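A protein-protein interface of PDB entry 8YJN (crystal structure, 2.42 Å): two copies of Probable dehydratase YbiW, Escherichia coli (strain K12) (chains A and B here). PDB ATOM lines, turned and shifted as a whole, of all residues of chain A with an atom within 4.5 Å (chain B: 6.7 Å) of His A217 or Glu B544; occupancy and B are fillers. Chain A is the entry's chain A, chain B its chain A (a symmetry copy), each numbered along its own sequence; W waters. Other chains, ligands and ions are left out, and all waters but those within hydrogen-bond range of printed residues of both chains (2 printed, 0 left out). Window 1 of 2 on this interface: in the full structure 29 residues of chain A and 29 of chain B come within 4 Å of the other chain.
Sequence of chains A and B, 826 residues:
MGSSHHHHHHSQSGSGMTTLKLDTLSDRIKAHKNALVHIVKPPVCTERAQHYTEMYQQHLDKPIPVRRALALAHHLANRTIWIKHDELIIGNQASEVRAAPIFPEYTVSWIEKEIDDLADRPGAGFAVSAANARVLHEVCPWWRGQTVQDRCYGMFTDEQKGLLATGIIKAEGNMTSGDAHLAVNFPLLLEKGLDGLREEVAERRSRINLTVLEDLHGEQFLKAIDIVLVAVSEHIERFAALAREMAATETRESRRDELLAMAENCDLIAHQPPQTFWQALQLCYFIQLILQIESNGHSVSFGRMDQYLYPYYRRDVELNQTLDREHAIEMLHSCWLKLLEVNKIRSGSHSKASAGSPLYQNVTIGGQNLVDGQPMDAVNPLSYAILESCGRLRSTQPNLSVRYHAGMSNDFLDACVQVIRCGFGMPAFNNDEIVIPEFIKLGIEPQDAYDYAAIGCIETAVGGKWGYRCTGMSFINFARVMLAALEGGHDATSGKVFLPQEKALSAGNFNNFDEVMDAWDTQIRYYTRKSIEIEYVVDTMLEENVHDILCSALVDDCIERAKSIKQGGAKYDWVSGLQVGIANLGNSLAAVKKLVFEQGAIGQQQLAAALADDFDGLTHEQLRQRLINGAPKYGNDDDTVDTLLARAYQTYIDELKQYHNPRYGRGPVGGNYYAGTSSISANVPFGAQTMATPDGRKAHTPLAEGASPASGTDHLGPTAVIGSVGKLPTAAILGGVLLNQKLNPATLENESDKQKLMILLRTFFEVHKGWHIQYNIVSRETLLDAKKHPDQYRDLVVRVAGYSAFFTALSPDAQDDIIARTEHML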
ATOM      1  N   LEU A 213       6.042   7.412  -3.276  1.00  0.00           N
ATOM      2  CA  LEU A 213       4.713   6.959  -2.874  1.00  0.00           C
ATOM      3  C   LEU A 213       4.768   5.579  -2.239  1.00  0.00           C
ATOM      4  O   LEU A 213       4.180   5.349  -1.175  1.00  0.00           O
ATOM      5  CB  LEU A 213       3.774   6.964  -4.072  1.00  0.00           C
ATOM      6  CG  LEU A 213       2.350   6.561  -3.710  1.00  0.00           C
ATOM      7  CD1 LEU A 213       1.793   7.451  -2.600  1.00  0.00           C
ATOM      8  CD2 LEU A 213       1.471   6.616  -4.933  1.00  0.00           C
ATOM      9  N   GLU A 214       5.498   4.653  -2.867  1.00  0.00           N
ATOM     10  CA  GLU A 214       5.569   3.286  -2.364  1.00  0.00           C
ATOM     11  C   GLU A 214       6.203   3.231  -0.980  1.00  0.00           C
ATOM     12  O   GLU A 214       5.839   2.371  -0.153  1.00  0.00           O
ATOM     13  CB  GLU A 214       6.365   2.412  -3.333  1.00  0.00           C
ATOM     14  CG  GLU A 214       5.498   1.580  -4.269  1.00  0.00           C
ATOM     15  CD  GLU A 214       6.265   1.041  -5.480  1.00  0.00           C
ATOM     16  OE1 GLU A 214       7.458   0.680  -5.311  1.00  0.00           O
ATOM     17  OE2 GLU A 214       5.665   0.962  -6.585  1.00  0.00           O
ATOM     18  N   ASP A 215       7.164   4.133  -0.716  1.00  0.00           N
ATOM     19  CA  ASP A 215       7.792   4.180   0.600  1.00  0.00           C
ATOM     20  C   ASP A 215       6.840   4.767   1.630  1.00  0.00           C
ATOM     21  O   ASP A 215       6.870   4.371   2.799  1.00  0.00           O
ATOM     22  CB  ASP A 215       9.086   5.003   0.559  1.00  0.00           C
ATOM     23  CG  ASP A 215      10.244   4.270  -0.113  1.00  0.00           C
ATOM     24  OD1 ASP A 215      10.047   3.142  -0.642  1.00  0.00           O
ATOM     25  OD2 ASP A 215      11.362   4.841  -0.105  1.00  0.00           O
ATOM     26  N   LEU A 216       6.003   5.729   1.224  1.00  0.00           N
ATOM     27  CA  LEU A 216       5.002   6.255   2.145  1.00  0.00           C
ATOM     28  C   LEU A 216       4.143   5.124   2.682  1.00  0.00           C
ATOM     29  O   LEU A 216       3.950   5.001   3.894  1.00  0.00           O
ATOM     30  CB  LEU A 216       4.134   7.319   1.457  1.00  0.00           C
ATOM     31  CG  LEU A 216       3.059   7.929   2.371  1.00  0.00           C
ATOM     32  CD1 LEU A 216       3.694   8.447   3.663  1.00  0.00           C
ATOM     33  CD2 LEU A 216       2.316   9.049   1.711  1.00  0.00           C
ATOM     34  N   HIS A 217       3.661   4.254   1.780  1.00  0.00           N
ATOM     35  CA  HIS A 217       2.865   3.098   2.180  1.00  0.00           C
ATOM     36  C   HIS A 217       3.705   2.056   2.895  1.00  0.00           C
ATOM     37  O   HIS A 217       3.254   1.468   3.882  1.00  0.00           O
ATOM     38  CB  HIS A 217       2.192   2.477   0.961  1.00  0.00           C
ATOM     39  CG  HIS A 217       1.108   3.327   0.391  1.00  0.00           C
ATOM     40  ND1 HIS A 217      -0.061   3.587   1.074  1.00  0.00           N
ATOM     41  CD2 HIS A 217       1.016   3.990  -0.788  1.00  0.00           C
ATOM     42  CE1 HIS A 217      -0.841   4.352   0.328  1.00  0.00           C
ATOM     43  NE2 HIS A 217      -0.211   4.611  -0.805  1.00  0.00           N
ATOM     44  N   GLY A 218       4.917   1.793   2.403  1.00  0.00           N
ATOM     45  CA  GLY A 218       5.763   0.827   3.076  1.00  0.00           C
ATOM     46  C   GLY A 218       6.034   1.219   4.511  1.00  0.00           C
ATOM     47  O   GLY A 218       5.998   0.378   5.412  1.00  0.00           O
ATOM     48  N   GLU A 219       6.259   2.517   4.748  1.00  0.00           N
ATOM     49  CA  GLU A 219       6.548   2.998   6.095  1.00  0.00           C
ATOM     50  C   GLU A 219       5.400   2.692   7.055  1.00  0.00           C
ATOM     51  O   GLU A 219       5.631   2.300   8.206  1.00  0.00           O
ATOM     52  CB  GLU A 219       6.865   4.510   6.039  1.00  0.00           C
ATOM     53  CG  GLU A 219       6.829   5.268   7.379  1.00  0.00           C
ATOM     54  CD  GLU A 219       7.786   4.706   8.449  1.00  0.00           C
ATOM     55  OE1 GLU A 219       8.732   3.938   8.120  1.00  0.00           O
ATOM     56  OE2 GLU A 219       7.572   5.033   9.640  1.00  0.00           O
ATOM     57  N   GLN A 220       4.154   2.859   6.601  1.00  0.00           N
ATOM     58  CA  GLN A 220       3.011   2.559   7.459  1.00  0.00           C
ATOM     59  C   GLN A 220       3.012   1.094   7.864  1.00  0.00           C
ATOM     60  O   GLN A 220       2.754   0.764   9.028  1.00  0.00           O
ATOM     61  CB  GLN A 220       1.694   2.903   6.753  1.00  0.00           C
ATOM     62  CG  GLN A 220       1.583   4.328   6.262  1.00  0.00           C
ATOM     63  CD  GLN A 220       2.046   5.338   7.292  1.00  0.00           C
ATOM     64  OE1 GLN A 220       1.656   5.276   8.469  1.00  0.00           O
ATOM     65  NE2 GLN A 220       2.903   6.266   6.860  1.00  0.00           N
ATOM     66  N   PHE A 221       3.311   0.201   6.909  1.00  0.00           N
ATOM     67  CA  PHE A 221       3.359  -1.221   7.227  1.00  0.00           C
ATOM     68  C   PHE A 221       4.542  -1.556   8.140  1.00  0.00           C
ATOM     69  O   PHE A 221       4.408  -2.353   9.076  1.00  0.00           O
ATOM     70  CB  PHE A 221       3.415  -2.055   5.944  1.00  0.00           C
ATOM     71  CG  PHE A 221       3.068  -3.479   6.184  1.00  0.00           C
ATOM     72  CD1 PHE A 221       1.758  -3.835   6.477  1.00  0.00           C
ATOM     73  CD2 PHE A 221       4.055  -4.455   6.216  1.00  0.00           C
ATOM     74  CE1 PHE A 221       1.436  -5.156   6.768  1.00  0.00           C
ATOM     75  CE2 PHE A 221       3.734  -5.772   6.491  1.00  0.00           C
ATOM     76  CZ  PHE A 221       2.415  -6.119   6.775  1.00  0.00           C
ATOM     77  N   ILE B  64     -15.256   2.695  -1.631  1.00  0.00           N
ATOM     78  CA  ILE B  64     -15.401   4.137  -1.410  1.00  0.00           C
ATOM     79  C   ILE B  64     -15.910   4.882  -2.650  1.00  0.00           C
ATOM     80  O   ILE B  64     -16.866   5.661  -2.521  1.00  0.00           O
ATOM     81  CB  ILE B  64     -14.104   4.717  -0.826  1.00  0.00           C
ATOM     82  CG1 ILE B  64     -14.007   4.357   0.664  1.00  0.00           C
ATOM     83  CG2 ILE B  64     -14.109   6.223  -0.869  1.00  0.00           C
ATOM     84  CD1 ILE B  64     -12.588   4.183   1.242  1.00  0.00           C
ATOM     85  N   PRO B  65     -15.376   4.668  -3.858  1.00  0.00           N
ATOM     86  CA  PRO B  65     -15.928   5.428  -5.002  1.00  0.00           C
ATOM     87  C   PRO B  65     -17.387   5.101  -5.262  1.00  0.00           C
ATOM     88  O   PRO B  65     -18.171   6.000  -5.602  1.00  0.00           O
ATOM     89  CB  PRO B  65     -15.020   5.030  -6.177  1.00  0.00           C
ATOM     90  CG  PRO B  65     -14.364   3.760  -5.745  1.00  0.00           C
ATOM     91  CD  PRO B  65     -14.216   3.855  -4.261  1.00  0.00           C
ATOM     92  N   ARG B 151      -7.359  11.729   8.941  1.00  0.00           N
ATOM     93  CA  ARG B 151      -6.511  10.664   8.431  1.00  0.00           C
ATOM     94  C   ARG B 151      -5.118  11.182   8.088  1.00  0.00           C
ATOM     95  O   ARG B 151      -4.132  10.444   8.246  1.00  0.00           O
ATOM     96  CB  ARG B 151      -7.189  10.000   7.240  1.00  0.00           C
ATOM     97  CG  ARG B 151      -8.496   9.305   7.649  1.00  0.00           C
ATOM     98  CD  ARG B 151      -8.533   7.889   7.193  1.00  0.00           C
ATOM     99  NE  ARG B 151      -9.350   7.062   8.067  1.00  0.00           N
ATOM    100  CZ  ARG B 151     -10.497   6.501   7.705  1.00  0.00           C
ATOM    101  NH1 ARG B 151     -10.975   6.632   6.476  1.00  0.00           N
ATOM    102  NH2 ARG B 151     -11.191   5.817   8.606  1.00  0.00           N
ATOM    103  N   MET B 155      -1.271   9.996  10.034  1.00  0.00           N
ATOM    104  CA  MET B 155      -0.158   9.455   9.262  1.00  0.00           C
ATOM    105  C   MET B 155       1.084  10.357   9.313  1.00  0.00           C
ATOM    106  O   MET B 155       2.206   9.864   9.180  1.00  0.00           O
ATOM    107  CB  MET B 155      -0.641   9.205   7.828  1.00  0.00           C
ATOM    108  CG  MET B 155       0.363   8.540   6.918  1.00  0.00           C
ATOM    109  SD  MET B 155      -0.319   8.294   5.266  1.00  0.00           S
ATOM    110  CE  MET B 155      -1.082   6.710   5.564  1.00  0.00           C
ATOM    111  N   ASP B 539      -2.165  14.372  -0.278  1.00  0.00           N
ATOM    112  CA  ASP B 539      -2.606  13.847  -1.564  1.00  0.00           C
ATOM    113  C   ASP B 539      -3.036  12.381  -1.439  1.00  0.00           C
ATOM    114  O   ASP B 539      -4.032  11.965  -2.039  1.00  0.00           O
ATOM    115  CB  ASP B 539      -1.482  13.989  -2.606  1.00  0.00           C
ATOM    116  CG  ASP B 539      -1.443  15.374  -3.280  1.00  0.00           C
ATOM    117  OD1 ASP B 539      -2.329  16.233  -3.029  1.00  0.00           O
ATOM    118  OD2 ASP B 539      -0.507  15.606  -4.085  1.00  0.00           O
ATOM    119  N   THR B 540      -2.317  11.589  -0.639  1.00  0.00           N
ATOM    120  CA  THR B 540      -2.636  10.165  -0.557  1.00  0.00           C
ATOM    121  C   THR B 540      -3.935   9.943   0.210  1.00  0.00           C
ATOM    122  O   THR B 540      -4.755   9.090  -0.160  1.00  0.00           O
ATOM    123  CB  THR B 540      -1.475   9.410   0.087  1.00  0.00           C
ATOM    124  OG1 THR B 540      -0.330   9.535  -0.762  1.00  0.00           O
ATOM    125  CG2 THR B 540      -1.808   7.924   0.243  1.00  0.00           C
ATOM    126  N   MET B 541      -4.155  10.737   1.257  1.00  0.00           N
ATOM    127  CA  MET B 541      -5.386  10.641   2.019  1.00  0.00           C
ATOM    128  C   MET B 541      -6.572  11.108   1.182  1.00  0.00           C
ATOM    129  O   MET B 541      -7.669  10.540   1.262  1.00  0.00           O
ATOM    130  CB  MET B 541      -5.221  11.459   3.293  1.00  0.00           C
ATOM    131  CG  MET B 541      -4.231  10.816   4.306  1.00  0.00           C
ATOM    132  SD  MET B 541      -4.547   9.058   4.646  1.00  0.00           S
ATOM    133  CE  MET B 541      -3.461   8.181   3.487  1.00  0.00           C
ATOM    134  N   LEU B 542      -6.357  12.127   0.348  1.00  0.00           N
ATOM    135  CA  LEU B 542      -7.398  12.515  -0.589  1.00  0.00           C
ATOM    136  C   LEU B 542      -7.643  11.403  -1.597  1.00  0.00           C
ATOM    137  O   LEU B 542      -8.796  11.093  -1.917  1.00  0.00           O
ATOM    138  CB  LEU B 542      -7.020  13.813  -1.310  1.00  0.00           C
ATOM    139  CG  LEU B 542      -6.969  15.169  -0.564  1.00  0.00           C
ATOM    140  CD1 LEU B 542      -6.073  16.185  -1.293  1.00  0.00           C
ATOM    141  CD2 LEU B 542      -8.347  15.785  -0.378  1.00  0.00           C
ATOM    142  N   GLU B 543      -6.561  10.800  -2.109  1.00  0.00           N
ATOM    143  CA  GLU B 543      -6.665   9.762  -3.127  1.00  0.00           C
ATOM    144  C   GLU B 543      -7.537   8.612  -2.652  1.00  0.00           C
ATOM    145  O   GLU B 543      -8.388   8.122  -3.401  1.00  0.00           O
ATOM    146  CB  GLU B 543      -5.274   9.241  -3.501  1.00  0.00           C
ATOM    147  CG  GLU B 543      -5.319   8.070  -4.469  1.00  0.00           C
ATOM    148  CD  GLU B 543      -3.961   7.493  -4.801  1.00  0.00           C
ATOM    149  OE1 GLU B 543      -2.936   8.017  -4.321  1.00  0.00           O
ATOM    150  OE2 GLU B 543      -3.909   6.526  -5.581  1.00  0.00           O
ATOM    151  N   GLU B 544      -7.364   8.205  -1.394  1.00  0.00           N
ATOM    152  CA  GLU B 544      -8.005   7.031  -0.824  1.00  0.00           C
ATOM    153  C   GLU B 544      -9.411   7.299  -0.311  1.00  0.00           C
ATOM    154  O   GLU B 544     -10.190   6.352  -0.178  1.00  0.00           O
ATOM    155  CB  GLU B 544      -7.160   6.485   0.335  1.00  0.00           C
ATOM    156  CG  GLU B 544      -5.814   5.943  -0.086  1.00  0.00           C
ATOM    157  CD  GLU B 544      -5.047   5.271   1.054  1.00  0.00           C
ATOM    158  OE1 GLU B 544      -5.497   5.329   2.226  1.00  0.00           O
ATOM    159  OE2 GLU B 544      -3.988   4.673   0.769  1.00  0.00           O
ATOM    160  N   ASN B 545      -9.753   8.549  -0.010  1.00  0.00           N
ATOM    161  CA  ASN B 545     -10.974   8.835   0.727  1.00  0.00           C
ATOM    162  C   ASN B 545     -12.011   9.645  -0.028  1.00  0.00           C
ATOM    163  O   ASN B 545     -13.205   9.486   0.256  1.00  0.00           O
ATOM    164  CB  ASN B 545     -10.642   9.571   2.027  1.00  0.00           C
ATOM    165  CG  ASN B 545      -9.988   8.663   3.044  1.00  0.00           C
ATOM    166  OD1 ASN B 545     -10.623   7.736   3.567  1.00  0.00           O
ATOM    167  ND2 ASN B 545      -8.711   8.916   3.328  1.00  0.00           N
ATOM    168  N   VAL B 546     -11.616  10.500  -0.970  1.00  0.00           N
ATOM    169  CA  VAL B 546     -12.595  11.421  -1.540  1.00  0.00           C
ATOM    170  C   VAL B 546     -12.510  11.501  -3.057  1.00  0.00           C
ATOM    171  O   VAL B 546     -12.474  12.602  -3.616  1.00  0.00           O
ATOM    172  CB  VAL B 546     -12.453  12.829  -0.932  1.00  0.00           C
ATOM    173  CG1 VAL B 546     -12.995  12.833   0.497  1.00  0.00           C
ATOM    174  CG2 VAL B 546     -10.980  13.324  -1.011  1.00  0.00           C
ATOM    175  N   HIS B 547     -12.505  10.347  -3.727  1.00  0.00           N
ATOM    176  CA  HIS B 547     -12.652  10.292  -5.179  1.00  0.00           C
ATOM    177  C   HIS B 547     -13.718  11.271  -5.671  1.00  0.00           C
ATOM    178  O   HIS B 547     -14.829  11.306  -5.133  1.00  0.00           O
ATOM    179  CB  HIS B 547     -13.053   8.873  -5.602  1.00  0.00           C
ATOM    180  CG  HIS B 547     -12.226   7.791  -4.993  1.00  0.00           C
ATOM    181  ND1 HIS B 547     -12.273   7.479  -3.648  1.00  0.00           N
ATOM    182  CD2 HIS B 547     -11.341   6.929  -5.548  1.00  0.00           C
ATOM    183  CE1 HIS B 547     -11.436   6.488  -3.399  1.00  0.00           C
ATOM    184  NE2 HIS B 547     -10.865   6.131  -4.537  1.00  0.00           N
ATOM    185  N   LYS B 566      -6.988  11.613  -8.986  1.00  0.00           N
ATOM    186  CA  LYS B 566      -6.004  11.514  -7.924  1.00  0.00           C
ATOM    187  C   LYS B 566      -5.227  10.202  -7.964  1.00  0.00           C
ATOM    188  O   LYS B 566      -4.181  10.093  -7.310  1.00  0.00           O
ATOM    189  CB  LYS B 566      -6.695  11.692  -6.572  1.00  0.00           C
ATOM    190  CG  LYS B 566      -5.782  12.264  -5.497  1.00  0.00           C
ATOM    191  CD  LYS B 566      -5.416  13.709  -5.791  1.00  0.00           C
ATOM    192  CE  LYS B 566      -4.494  14.273  -4.715  1.00  0.00           C
ATOM    193  NZ  LYS B 566      -4.321  15.757  -4.871  1.00  0.00           N
ATOM    194  N   GLN B 567      -5.706   9.201  -8.701  1.00  0.00           N
ATOM    195  CA  GLN B 567      -4.977   7.945  -8.804  1.00  0.00           C
ATOM    196  C   GLN B 567      -4.053   7.906 -10.015  1.00  0.00           C
ATOM    197  O   GLN B 567      -3.352   6.904 -10.209  1.00  0.00           O
ATOM    198  CB  GLN B 567      -5.943   6.763  -8.867  1.00  0.00           C
ATOM    199  CG  GLN B 567      -6.819   6.605  -7.663  1.00  0.00           C
ATOM    200  CD  GLN B 567      -7.822   5.464  -7.826  1.00  0.00           C
ATOM    201  OE1 GLN B 567      -8.893   5.638  -8.413  1.00  0.00           O
ATOM    202  NE2 GLN B 567      -7.473   4.289  -7.303  1.00  0.00           N
ATOM    203  N   ARG B 666       2.301   6.709 -12.682  1.00  0.00           N
ATOM    204  CA  ARG B 666       1.041   6.011 -12.486  1.00  0.00           C
ATOM    205  C   ARG B 666       0.036   6.366 -13.575  1.00  0.00           C
ATOM    206  O   ARG B 666      -1.165   6.151 -13.409  1.00  0.00           O
ATOM    207  CB  ARG B 666       0.491   6.306 -11.086  1.00  0.00           C
ATOM    208  CG  ARG B 666       1.422   5.898  -9.929  1.00  0.00           C
ATOM    209  CD  ARG B 666       0.640   5.565  -8.647  1.00  0.00           C
ATOM    210  NE  ARG B 666       0.232   6.790  -7.967  1.00  0.00           N
ATOM    211  CZ  ARG B 666      -0.901   6.930  -7.295  1.00  0.00           C
ATOM    212  NH1 ARG B 666      -1.713   5.899  -7.097  1.00  0.00           N
ATOM    213  NH2 ARG B 666      -1.225   8.131  -6.808  1.00  0.00           N
HETATM  214  O   HOH W   1       5.050   8.339   8.045  1.00  0.00           O
HETATM  215  O   HOH W   2      -1.620   5.713  -3.033  1.00  0.00           O
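Water W2 lies within hydrogen-bond range of a ring nitrogen (NE2) of His A217 (2.9 Å) and the side-chain carboxylate of Glu B543 (2.9 Å).
Water W1 bridges the side-chain amide nitrogen of Gln A220 and the backbone carbonyl oxygen of Met B155.
Of the printed residues of chain B, Leu A213 touches Thr B540 (3.5 Å) and Arg B666 (3.3 Å).
Of the printed residues of chain B, Leu A216 touches Thr B540.
His A217 touches just these residues of chain B: Thr B540 (3.7 Å) and Glu B544 (3.2 Å).
Of the printed residues of chain B, Gln A220 touches Met B155.
Glu B544 touches one residue of chain A.
Of the printed residues of chain A, Arg B666 touches Leu A213 (3.3 Å).
The nearest residue of chain B that does not touch His A217 is Met B155 (5.6 Å).
The nearest printed residue of chain A that does not touch Glu B544 is Leu A213 (7.2 Å).
The nearest printed residue of chain A that does not touch Thr B540 is Gln A220 (7.8 Å).
Of the 9 printed residues of chain A, 4 touch a printed residue of chain B.
Hydrophobic or aromatic side chains of chain A within 4 Å of the printed part of chain B: Leu A213, Leu A216 and His A217.
Of the 16 printed residues of chain B, 4 touch a printed residue of chain A.
Along chain B the printed residues that touch a printed residue of chain A span positions 155 to 666.
No position is printed for both chains.
Leu A213 touches Thr B540 (CD1 to OG1, 3.5 Å).
Arg B666 touches Leu A213.
CD2 of Leu A216 touches OG1 of Thr B540 (3.7 Å).
Thr B540 touches His A217 (CG2 to CE1, 3.7 Å).
Glu B544 touches His A217 (OE2 to CE1, 3.2 Å).
NE2 of Gln A220 touches CG of Met B155, at 3.4 Å.
The side-chain amide nitrogen of Gln A220 sits at hydrogen-bond distance from the backbone carbonyl oxygen of Leu A216 (3.4 Å).
OE2 of Glu B543 is in salt-bridge range of NH1 of Arg B666 (2.7 Å).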
